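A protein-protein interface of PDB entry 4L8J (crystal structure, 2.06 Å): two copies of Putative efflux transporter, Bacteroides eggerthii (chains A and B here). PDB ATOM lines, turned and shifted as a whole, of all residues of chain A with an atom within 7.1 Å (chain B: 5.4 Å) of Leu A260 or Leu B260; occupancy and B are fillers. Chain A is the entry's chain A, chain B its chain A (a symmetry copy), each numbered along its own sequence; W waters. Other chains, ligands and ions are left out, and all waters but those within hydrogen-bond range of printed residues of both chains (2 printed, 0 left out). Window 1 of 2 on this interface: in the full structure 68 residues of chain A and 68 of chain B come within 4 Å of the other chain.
N of Leu A298 sits at hydrogen-bond distance from O of Val B258, at 2.8 Å.
N of Leu B260 is in hydrogen-bond range of O of Ala A296 (2.9 Å).
The side-chain hydroxyl (OG) of Ser B261 sits at hydrogen-bond distance from the backbone carbonyl oxygen (O) of Thr A312 (2.7 Å).
The backbone carbonyl oxygen (O) of Val A258 is in hydrogen-bond range of the backbone NH (N) of Leu B298.
N of Leu A260 sits at hydrogen-bond distance from O of Ala B296 (2.9 Å).
The side-chain amide nitrogen of Asn A297 sits at hydrogen-bond distance from the backbone carbonyl oxygen of Glu A295 (2.8 Å).
Among the printed residues, merely in contact across the chains: Val A258 with Asn B297 (3.6 Å), Asn A297 with Val B258 (3.6 Å), Asn A297 with Pro B259 (3.6 Å), Pro A259 with Asn B297 (3.6 Å), Leu A260 with Leu B260 (3.6 Å), Pro A259 with Ala B296 (3.7 Å), Ala A296 with Pro B259 (3.7 Å), Val A263 with Leu B298 (3.7 Å), Leu A298 with Val B263 (3.7 Å), Thr A312 with Pro B259 (3.7 Å), Leu A260 with Leu B298 (3.9 Å), Leu A298 with Leu B260 (3.9 Å), Leu A260 with Val B289 (3.96 Å), Val A289 with Leu B260 (3.96 Å), Leu A260 with Asn B297 (3.97 Å) and Asn A297 with Leu B260 (3.97 Å).
Of the printed residues of chain B, Leu A260 touches Leu B260, Val B289, Ala B296, Asn B297 and Leu B298.
Thr A272 touches none of the printed residues of chain B.
Of the printed residues of chain B, Asn A297 touches Val B258 (3.6 Å), Pro B259 (3.6 Å) and Leu B260 (3.97 Å).
Of the printed residues of chain B, Leu A298 touches Val B258 (2.8 Å), Leu B260 (3.9 Å) and Val B263 (3.7 Å).
Of the printed residues of chain A, Leu B260 touches Leu A260 (3.6 Å), Val A289 (3.96 Å), Ala A296 (2.9 Å), Asn A297 (3.97 Å) and Leu A298 (3.9 Å).
Of the printed residues of chain A, Val B263 touches Leu A298.
Of the printed residues of chain A, Ala B296 touches Pro A259 (3.7 Å) and Leu A260 (2.9 Å).
The nearest printed residue of chain B that does not touch Leu A260 is Thr B272 (4.5 Å).
The nearest printed residue of chain B that does not touch Ala A296 is Ser B261 (4.8 Å).
Hydrophobic or aromatic side chains of chain B within 4 Å of the printed part of chain A: Pro B259, Leu B260, Val B263, Val B289 and Leu B298.
Printed residues of chain A that touch a printed residue of chain B: Val A258, Pro A259, Leu A260, Val A263, Val A289, Ala A296, Asn A297, Leu A298 and Thr A312.
Hydrophobic or aromatic side chains of chain A within 4 Å of the printed part of chain B: Pro A259, Leu A260, Val A263, Val A289 and Leu A298.
Along chain A the printed residues that touch a printed residue of chain B span positions 258 to 312.
Among the printed residues, no Asp or Glu carboxylate lies within 4 Å of a Lys or Arg side-chain nitrogen of the other chain.
Val A258 touches Leu B298, and with the chains exchanged Leu A298 touches Val B258.
Leu A260 touches Val B289, and with the chains exchanged Val A289 touches Leu B260.
Leu A260 touches Leu B298, and with the chains exchanged Leu A298 touches Leu B260.
Val A263 touches Leu B298, and with the chains exchanged Leu A298 touches Val B263.
Water W2 lies within hydrogen-bond range of O of Ala B296 (2.8 Å), N of Ser A261 (3.0 Å) and N of Leu A260 (3.1 Å).
Water W1 lies within hydrogen-bond range of O of Ala A296, N of Ser B261 and N of Leu B260.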
ATOM      1  N   VAL A 258     -22.946   3.191 -13.533  1.00  0.00           N
ATOM      2  CA  VAL A 258     -22.236   2.295 -14.439  1.00  0.00           C
ATOM      3  C   VAL A 258     -20.771   2.275 -14.026  1.00  0.00           C
ATOM      4  O   VAL A 258     -20.250   3.344 -13.696  1.00  0.00           O
ATOM      5  CB  VAL A 258     -22.371   2.571 -15.971  1.00  0.00           C
ATOM      6  CG1 VAL A 258     -23.809   2.478 -16.450  1.00  0.00           C
ATOM      7  CG2 VAL A 258     -21.720   3.882 -16.396  1.00  0.00           C
ATOM      8  N   PRO A 259     -20.043   1.139 -14.126  1.00  0.00           N
ATOM      9  CA  PRO A 259     -18.593   1.184 -13.854  1.00  0.00           C
ATOM     10  C   PRO A 259     -17.879   2.118 -14.834  1.00  0.00           C
ATOM     11  O   PRO A 259     -18.318   2.293 -15.982  1.00  0.00           O
ATOM     12  CB  PRO A 259     -18.151  -0.272 -14.084  1.00  0.00           C
ATOM     13  CG  PRO A 259     -19.394  -1.084 -13.761  1.00  0.00           C
ATOM     14  CD  PRO A 259     -20.478  -0.236 -14.428  1.00  0.00           C
ATOM     15  N   LEU A 260     -16.795   2.739 -14.388  1.00  0.00           N
ATOM     16  CA  LEU A 260     -15.997   3.611 -15.252  1.00  0.00           C
ATOM     17  C   LEU A 260     -15.529   2.830 -16.497  1.00  0.00           C
ATOM     18  O   LEU A 260     -15.562   3.370 -17.603  1.00  0.00           O
ATOM     19  CB  LEU A 260     -14.788   4.164 -14.464  1.00  0.00           C
ATOM     20  CG  LEU A 260     -13.664   4.826 -15.245  1.00  0.00           C
ATOM     21  CD1 LEU A 260     -14.141   6.103 -15.888  1.00  0.00           C
ATOM     22  CD2 LEU A 260     -12.454   5.096 -14.354  1.00  0.00           C
ATOM     23  N   SER A 261     -15.140   1.548 -16.314  1.00  0.00           N
ATOM     24  CA  SER A 261     -14.622   0.700 -17.398  1.00  0.00           C
ATOM     25  C   SER A 261     -15.669   0.452 -18.530  1.00  0.00           C
ATOM     26  O   SER A 261     -15.313  -0.051 -19.590  1.00  0.00           O
ATOM     27  CB  SER A 261     -14.103  -0.614 -16.826  1.00  0.00           C
ATOM     28  OG  SER A 261     -15.166  -1.414 -16.335  1.00  0.00           O
ATOM     29  N   ALA A 262     -16.939   0.813 -18.313  1.00  0.00           N
ATOM     30  CA  ALA A 262     -17.984   0.674 -19.335  1.00  0.00           C
ATOM     31  C   ALA A 262     -17.976   1.842 -20.328  1.00  0.00           C
ATOM     32  O   ALA A 262     -18.459   1.688 -21.451  1.00  0.00           O
ATOM     33  CB  ALA A 262     -19.363   0.591 -18.675  1.00  0.00           C
ATOM     34  N   VAL A 263     -17.460   3.012 -19.905  1.00  0.00           N
ATOM     35  CA  VAL A 263     -17.546   4.229 -20.682  1.00  0.00           C
ATOM     36  C   VAL A 263     -16.289   4.456 -21.549  1.00  0.00           C
ATOM     37  O   VAL A 263     -15.152   4.258 -21.106  1.00  0.00           O
ATOM     38  CB  VAL A 263     -17.856   5.447 -19.745  1.00  0.00           C
ATOM     39  CG1 VAL A 263     -17.930   6.764 -20.518  1.00  0.00           C
ATOM     40  CG2 VAL A 263     -19.154   5.226 -18.962  1.00  0.00           C
ATOM     41  N   PHE A 264     -16.526   4.876 -22.806  1.00  0.00           N
ATOM     42  CA  PHE A 264     -15.466   5.160 -23.765  1.00  0.00           C
ATOM     43  C   PHE A 264     -15.836   6.383 -24.629  1.00  0.00           C
ATOM     44  O   PHE A 264     -16.998   6.821 -24.650  1.00  0.00           O
ATOM     45  CB  PHE A 264     -15.165   3.913 -24.634  1.00  0.00           C
ATOM     46  CG  PHE A 264     -16.336   3.343 -25.396  1.00  0.00           C
ATOM     47  CD1 PHE A 264     -17.142   2.359 -24.829  1.00  0.00           C
ATOM     48  CD2 PHE A 264     -16.618   3.768 -26.687  1.00  0.00           C
ATOM     49  CE1 PHE A 264     -18.219   1.821 -25.542  1.00  0.00           C
ATOM     50  CE2 PHE A 264     -17.678   3.210 -27.406  1.00  0.00           C
ATOM     51  CZ  PHE A 264     -18.474   2.244 -26.824  1.00  0.00           C
ATOM     52  N   THR A 272     -19.452  10.640 -24.876  1.00  0.00           N
ATOM     53  CA  THR A 272     -19.188   9.419 -24.103  1.00  0.00           C
ATOM     54  C   THR A 272     -20.215   8.373 -24.470  1.00  0.00           C
ATOM     55  O   THR A 272     -21.379   8.688 -24.680  1.00  0.00           O
ATOM     56  CB  THR A 272     -19.150   9.700 -22.604  1.00  0.00           C
ATOM     57  OG1 THR A 272     -20.364  10.352 -22.209  1.00  0.00           O
ATOM     58  CG2 THR A 272     -17.914  10.519 -22.206  1.00  0.00           C
ATOM     59  N   TYR A 273     -19.767   7.121 -24.542  1.00  0.00           N
ATOM     60  CA  TYR A 273     -20.583   5.978 -24.933  1.00  0.00           C
ATOM     61  C   TYR A 273     -20.398   4.795 -24.020  1.00  0.00           C
ATOM     62  O   TYR A 273     -19.413   4.706 -23.291  1.00  0.00           O
ATOM     63  CB  TYR A 273     -20.201   5.530 -26.379  1.00  0.00           C
ATOM     64  CG  TYR A 273     -20.273   6.635 -27.407  1.00  0.00           C
ATOM     65  CD1 TYR A 273     -21.459   6.908 -28.087  1.00  0.00           C
ATOM     66  CD2 TYR A 273     -19.164   7.435 -27.679  1.00  0.00           C
ATOM     67  CE1 TYR A 273     -21.541   7.956 -29.005  1.00  0.00           C
ATOM     68  CE2 TYR A 273     -19.238   8.486 -28.590  1.00  0.00           C
ATOM     69  CZ  TYR A 273     -20.420   8.724 -29.274  1.00  0.00           C
ATOM     70  OH  TYR A 273     -20.480   9.756 -30.182  1.00  0.00           O
ATOM     71  N   VAL A 289     -22.360  11.751 -18.765  1.00  0.00           N
ATOM     72  CA  VAL A 289     -21.784  11.532 -17.452  1.00  0.00           C
ATOM     73  C   VAL A 289     -22.185  12.734 -16.591  1.00  0.00           C
ATOM     74  O   VAL A 289     -22.052  13.881 -17.036  1.00  0.00           O
ATOM     75  CB  VAL A 289     -20.243  11.301 -17.506  1.00  0.00           C
ATOM     76  CG1 VAL A 289     -19.650  11.148 -16.100  1.00  0.00           C
ATOM     77  CG2 VAL A 289     -19.902  10.084 -18.350  1.00  0.00           C
ATOM     78  N   GLU A 295     -17.060  20.071 -17.380  1.00  0.00           N
ATOM     79  CA  GLU A 295     -16.723  18.739 -17.885  1.00  0.00           C
ATOM     80  C   GLU A 295     -16.399  17.787 -16.729  1.00  0.00           C
ATOM     81  O   GLU A 295     -15.778  18.213 -15.752  1.00  0.00           O
ATOM     82  CB  GLU A 295     -15.550  18.809 -18.882  1.00  0.00           C
ATOM     83  CG  GLU A 295     -15.802  19.683 -20.111  1.00  0.00           C
ATOM     84  CD  GLU A 295     -16.944  19.303 -21.043  1.00  0.00           C
ATOM     85  OE1 GLU A 295     -17.287  18.099 -21.135  1.00  0.00           O
ATOM     86  OE2 GLU A 295     -17.473  20.219 -21.716  1.00  0.00           O
ATOM     87  N   ALA A 296     -16.823  16.505 -16.835  1.00  0.00           N
ATOM     88  CA  ALA A 296     -16.588  15.508 -15.781  1.00  0.00           C
ATOM     89  C   ALA A 296     -15.084  15.356 -15.479  1.00  0.00           C
ATOM     90  O   ALA A 296     -14.261  15.275 -16.401  1.00  0.00           O
ATOM     91  CB  ALA A 296     -17.193  14.166 -16.168  1.00  0.00           C
ATOM     92  N   ASN A 297     -14.758  15.341 -14.177  1.00  0.00           N
ATOM     93  CA  ASN A 297     -13.381  15.174 -13.692  1.00  0.00           C
ATOM     94  C   ASN A 297     -13.271  13.943 -12.801  1.00  0.00           C
ATOM     95  O   ASN A 297     -14.260  13.515 -12.189  1.00  0.00           O
ATOM     96  CB  ASN A 297     -12.874  16.409 -12.934  1.00  0.00           C
ATOM     97  CG  ASN A 297     -12.775  17.645 -13.778  1.00  0.00           C
ATOM     98  OD1 ASN A 297     -11.736  17.938 -14.396  1.00  0.00           O
ATOM     99  ND2 ASN A 297     -13.848  18.419 -13.778  1.00  0.00           N
ATOM    100  N   LEU A 298     -12.049  13.359 -12.746  1.00  0.00           N
ATOM    101  CA  LEU A 298     -11.731  12.190 -11.929  1.00  0.00           C
ATOM    102  C   LEU A 298     -10.713  12.551 -10.851  1.00  0.00           C
ATOM    103  O   LEU A 298      -9.818  13.382 -11.059  1.00  0.00           O
ATOM    104  CB  LEU A 298     -11.158  11.025 -12.773  1.00  0.00           C
ATOM    105  CG  LEU A 298     -12.092  10.310 -13.760  1.00  0.00           C
ATOM    106  CD1 LEU A 298     -11.332   9.195 -14.487  1.00  0.00           C
ATOM    107  CD2 LEU A 298     -13.333   9.696 -13.033  1.00  0.00           C
ATOM    108  N   THR A 312      -6.076  15.817 -22.985  1.00  0.00           N
ATOM    109  CA  THR A 312      -7.510  15.730 -22.660  1.00  0.00           C
ATOM    110  C   THR A 312      -8.387  15.526 -23.922  1.00  0.00           C
ATOM    111  O   THR A 312      -9.579  15.253 -23.794  1.00  0.00           O
ATOM    112  CB  THR A 312      -7.961  16.962 -21.883  1.00  0.00           C
ATOM    113  OG1 THR A 312      -7.761  18.124 -22.697  1.00  0.00           O
ATOM    114  CG2 THR A 312      -7.232  17.110 -20.568  1.00  0.00           C
ATOM    115  N   VAL B 258      -7.939  15.262 -12.729  1.00  0.00           N
ATOM    116  CA  VAL B 258      -7.733  15.177 -14.171  1.00  0.00           C
ATOM    117  C   VAL B 258      -9.102  15.091 -14.835  1.00  0.00           C
ATOM    118  O   VAL B 258      -9.960  14.384 -14.300  1.00  0.00           O
ATOM    119  CB  VAL B 258      -6.797  14.041 -14.695  1.00  0.00           C
ATOM    120  CG1 VAL B 258      -5.384  14.161 -14.151  1.00  0.00           C
ATOM    121  CG2 VAL B 258      -7.372  12.648 -14.466  1.00  0.00           C
ATOM    122  N   PRO B 259      -9.325  15.686 -16.029  1.00  0.00           N
ATOM    123  CA  PRO B 259     -10.613  15.468 -16.715  1.00  0.00           C
ATOM    124  C   PRO B 259     -10.817  13.988 -17.043  1.00  0.00           C
ATOM    125  O   PRO B 259      -9.847  13.243 -17.258  1.00  0.00           O
ATOM    126  CB  PRO B 259     -10.461  16.287 -18.009  1.00  0.00           C
ATOM    127  CG  PRO B 259      -9.493  17.394 -17.626  1.00  0.00           C
ATOM    128  CD  PRO B 259      -8.473  16.615 -16.793  1.00  0.00           C
ATOM    129  N   LEU B 260     -12.067  13.545 -17.063  1.00  0.00           N
ATOM    130  CA  LEU B 260     -12.389  12.162 -17.420  1.00  0.00           C
ATOM    131  C   LEU B 260     -11.827  11.838 -18.819  1.00  0.00           C
ATOM    132  O   LEU B 260     -11.283  10.751 -19.021  1.00  0.00           O
ATOM    133  CB  LEU B 260     -13.920  11.954 -17.383  1.00  0.00           C
ATOM    134  CG  LEU B 260     -14.490  10.698 -18.022  1.00  0.00           C
ATOM    135  CD1 LEU B 260     -14.059   9.470 -17.263  1.00  0.00           C
ATOM    136  CD2 LEU B 260     -16.012  10.764 -18.111  1.00  0.00           C
ATOM    137  N   SER B 261     -11.918  12.802 -19.763  1.00  0.00           N
ATOM    138  CA  SER B 261     -11.472  12.616 -21.152  1.00  0.00           C
ATOM    139  C   SER B 261      -9.939  12.342 -21.267  1.00  0.00           C
ATOM    140  O   SER B 261      -9.466  11.957 -22.331  1.00  0.00           O
ATOM    141  CB  SER B 261     -11.886  13.816 -21.994  1.00  0.00           C
ATOM    142  OG  SER B 261     -11.158  14.976 -21.625  1.00  0.00           O
ATOM    143  N   ALA B 262      -9.177  12.526 -20.183  1.00  0.00           N
ATOM    144  CA  ALA B 262      -7.736  12.240 -20.176  1.00  0.00           C
ATOM    145  C   ALA B 262      -7.446  10.751 -19.948  1.00  0.00           C
ATOM    146  O   ALA B 262      -6.375  10.277 -20.331  1.00  0.00           O
ATOM    147  CB  ALA B 262      -7.041  13.057 -19.082  1.00  0.00           C
ATOM    148  N   VAL B 263      -8.379  10.030 -19.299  1.00  0.00           N
ATOM    149  CA  VAL B 263      -8.156   8.665 -18.875  1.00  0.00           C
ATOM    150  C   VAL B 263      -8.671   7.642 -19.911  1.00  0.00           C
ATOM    151  O   VAL B 263      -9.759   7.789 -20.479  1.00  0.00           O
ATOM    152  CB  VAL B 263      -8.767   8.435 -17.451  1.00  0.00           C
ATOM    153  CG1 VAL B 263      -8.579   6.996 -16.970  1.00  0.00           C
ATOM    154  CG2 VAL B 263      -8.171   9.410 -16.430  1.00  0.00           C
ATOM    155  N   THR B 272      -5.797   1.769 -15.842  1.00  0.00           N
ATOM    156  CA  THR B 272      -6.155   3.090 -16.375  1.00  0.00           C
ATOM    157  C   THR B 272      -4.890   3.882 -16.617  1.00  0.00           C
ATOM    158  O   THR B 272      -3.946   3.803 -15.841  1.00  0.00           O
ATOM    159  CB  THR B 272      -7.134   3.819 -15.461  1.00  0.00           C
ATOM    160  OG1 THR B 272      -6.590   3.886 -14.135  1.00  0.00           O
ATOM    161  CG2 THR B 272      -8.522   3.163 -15.468  1.00  0.00           C
ATOM    162  N   VAL B 289      -7.419   5.516 -10.333  1.00  0.00           N
ATOM    163  CA  VAL B 289      -8.581   6.364 -10.144  1.00  0.00           C
ATOM    164  C   VAL B 289      -9.074   6.119  -8.714  1.00  0.00           C
ATOM    165  O   VAL B 289      -9.196   4.962  -8.295  1.00  0.00           O
ATOM    166  CB  VAL B 289      -9.681   6.121 -11.222  1.00  0.00           C
ATOM    167  CG1 VAL B 289     -10.927   6.974 -10.954  1.00  0.00           C
ATOM    168  CG2 VAL B 289      -9.149   6.401 -12.617  1.00  0.00           C
ATOM    169  N   ALA B 296     -13.990   1.871  -9.612  1.00  0.00           N
ATOM    170  CA  ALA B 296     -14.546   3.212  -9.844  1.00  0.00           C
ATOM    171  C   ALA B 296     -15.846   3.145 -10.670  1.00  0.00           C
ATOM    172  O   ALA B 296     -15.918   2.421 -11.673  1.00  0.00           O
ATOM    173  CB  ALA B 296     -13.522   4.105 -10.530  1.00  0.00           C
ATOM    174  N   ASN B 297     -16.858   3.896 -10.210  1.00  0.00           N
ATOM    175  CA  ASN B 297     -18.164   3.986 -10.880  1.00  0.00           C
ATOM    176  C   ASN B 297     -18.470   5.427 -11.267  1.00  0.00           C
ATOM    177  O   ASN B 297     -17.962   6.371 -10.645  1.00  0.00           O
ATOM    178  CB  ASN B 297     -19.304   3.430 -10.014  1.00  0.00           C
ATOM    179  CG  ASN B 297     -19.188   1.963  -9.721  1.00  0.00           C
ATOM    180  OD1 ASN B 297     -19.698   1.103 -10.461  1.00  0.00           O
ATOM    181  ND2 ASN B 297     -18.550   1.657  -8.603  1.00  0.00           N
ATOM    182  N   LEU B 298     -19.301   5.592 -12.326  1.00  0.00           N
ATOM    183  CA  LEU B 298     -19.738   6.890 -12.835  1.00  0.00           C
ATOM    184  C   LEU B 298     -21.245   7.053 -12.659  1.00  0.00           C
ATOM    185  O   LEU B 298     -22.017   6.090 -12.767  1.00  0.00           O
ATOM    186  CB  LEU B 298     -19.397   7.075 -14.334  1.00  0.00           C
ATOM    187  CG  LEU B 298     -17.922   7.209 -14.737  1.00  0.00           C
ATOM    188  CD1 LEU B 298     -17.806   7.385 -16.254  1.00  0.00           C
ATOM    189  CD2 LEU B 298     -17.242   8.425 -14.026  1.00  0.00           C
HETATM  190  O   HOH W   1     -13.867  15.051 -19.154  1.00  0.00           O
HETATM  191  O   HOH W   2     -14.549   0.754 -13.443  1.00  0.00           O
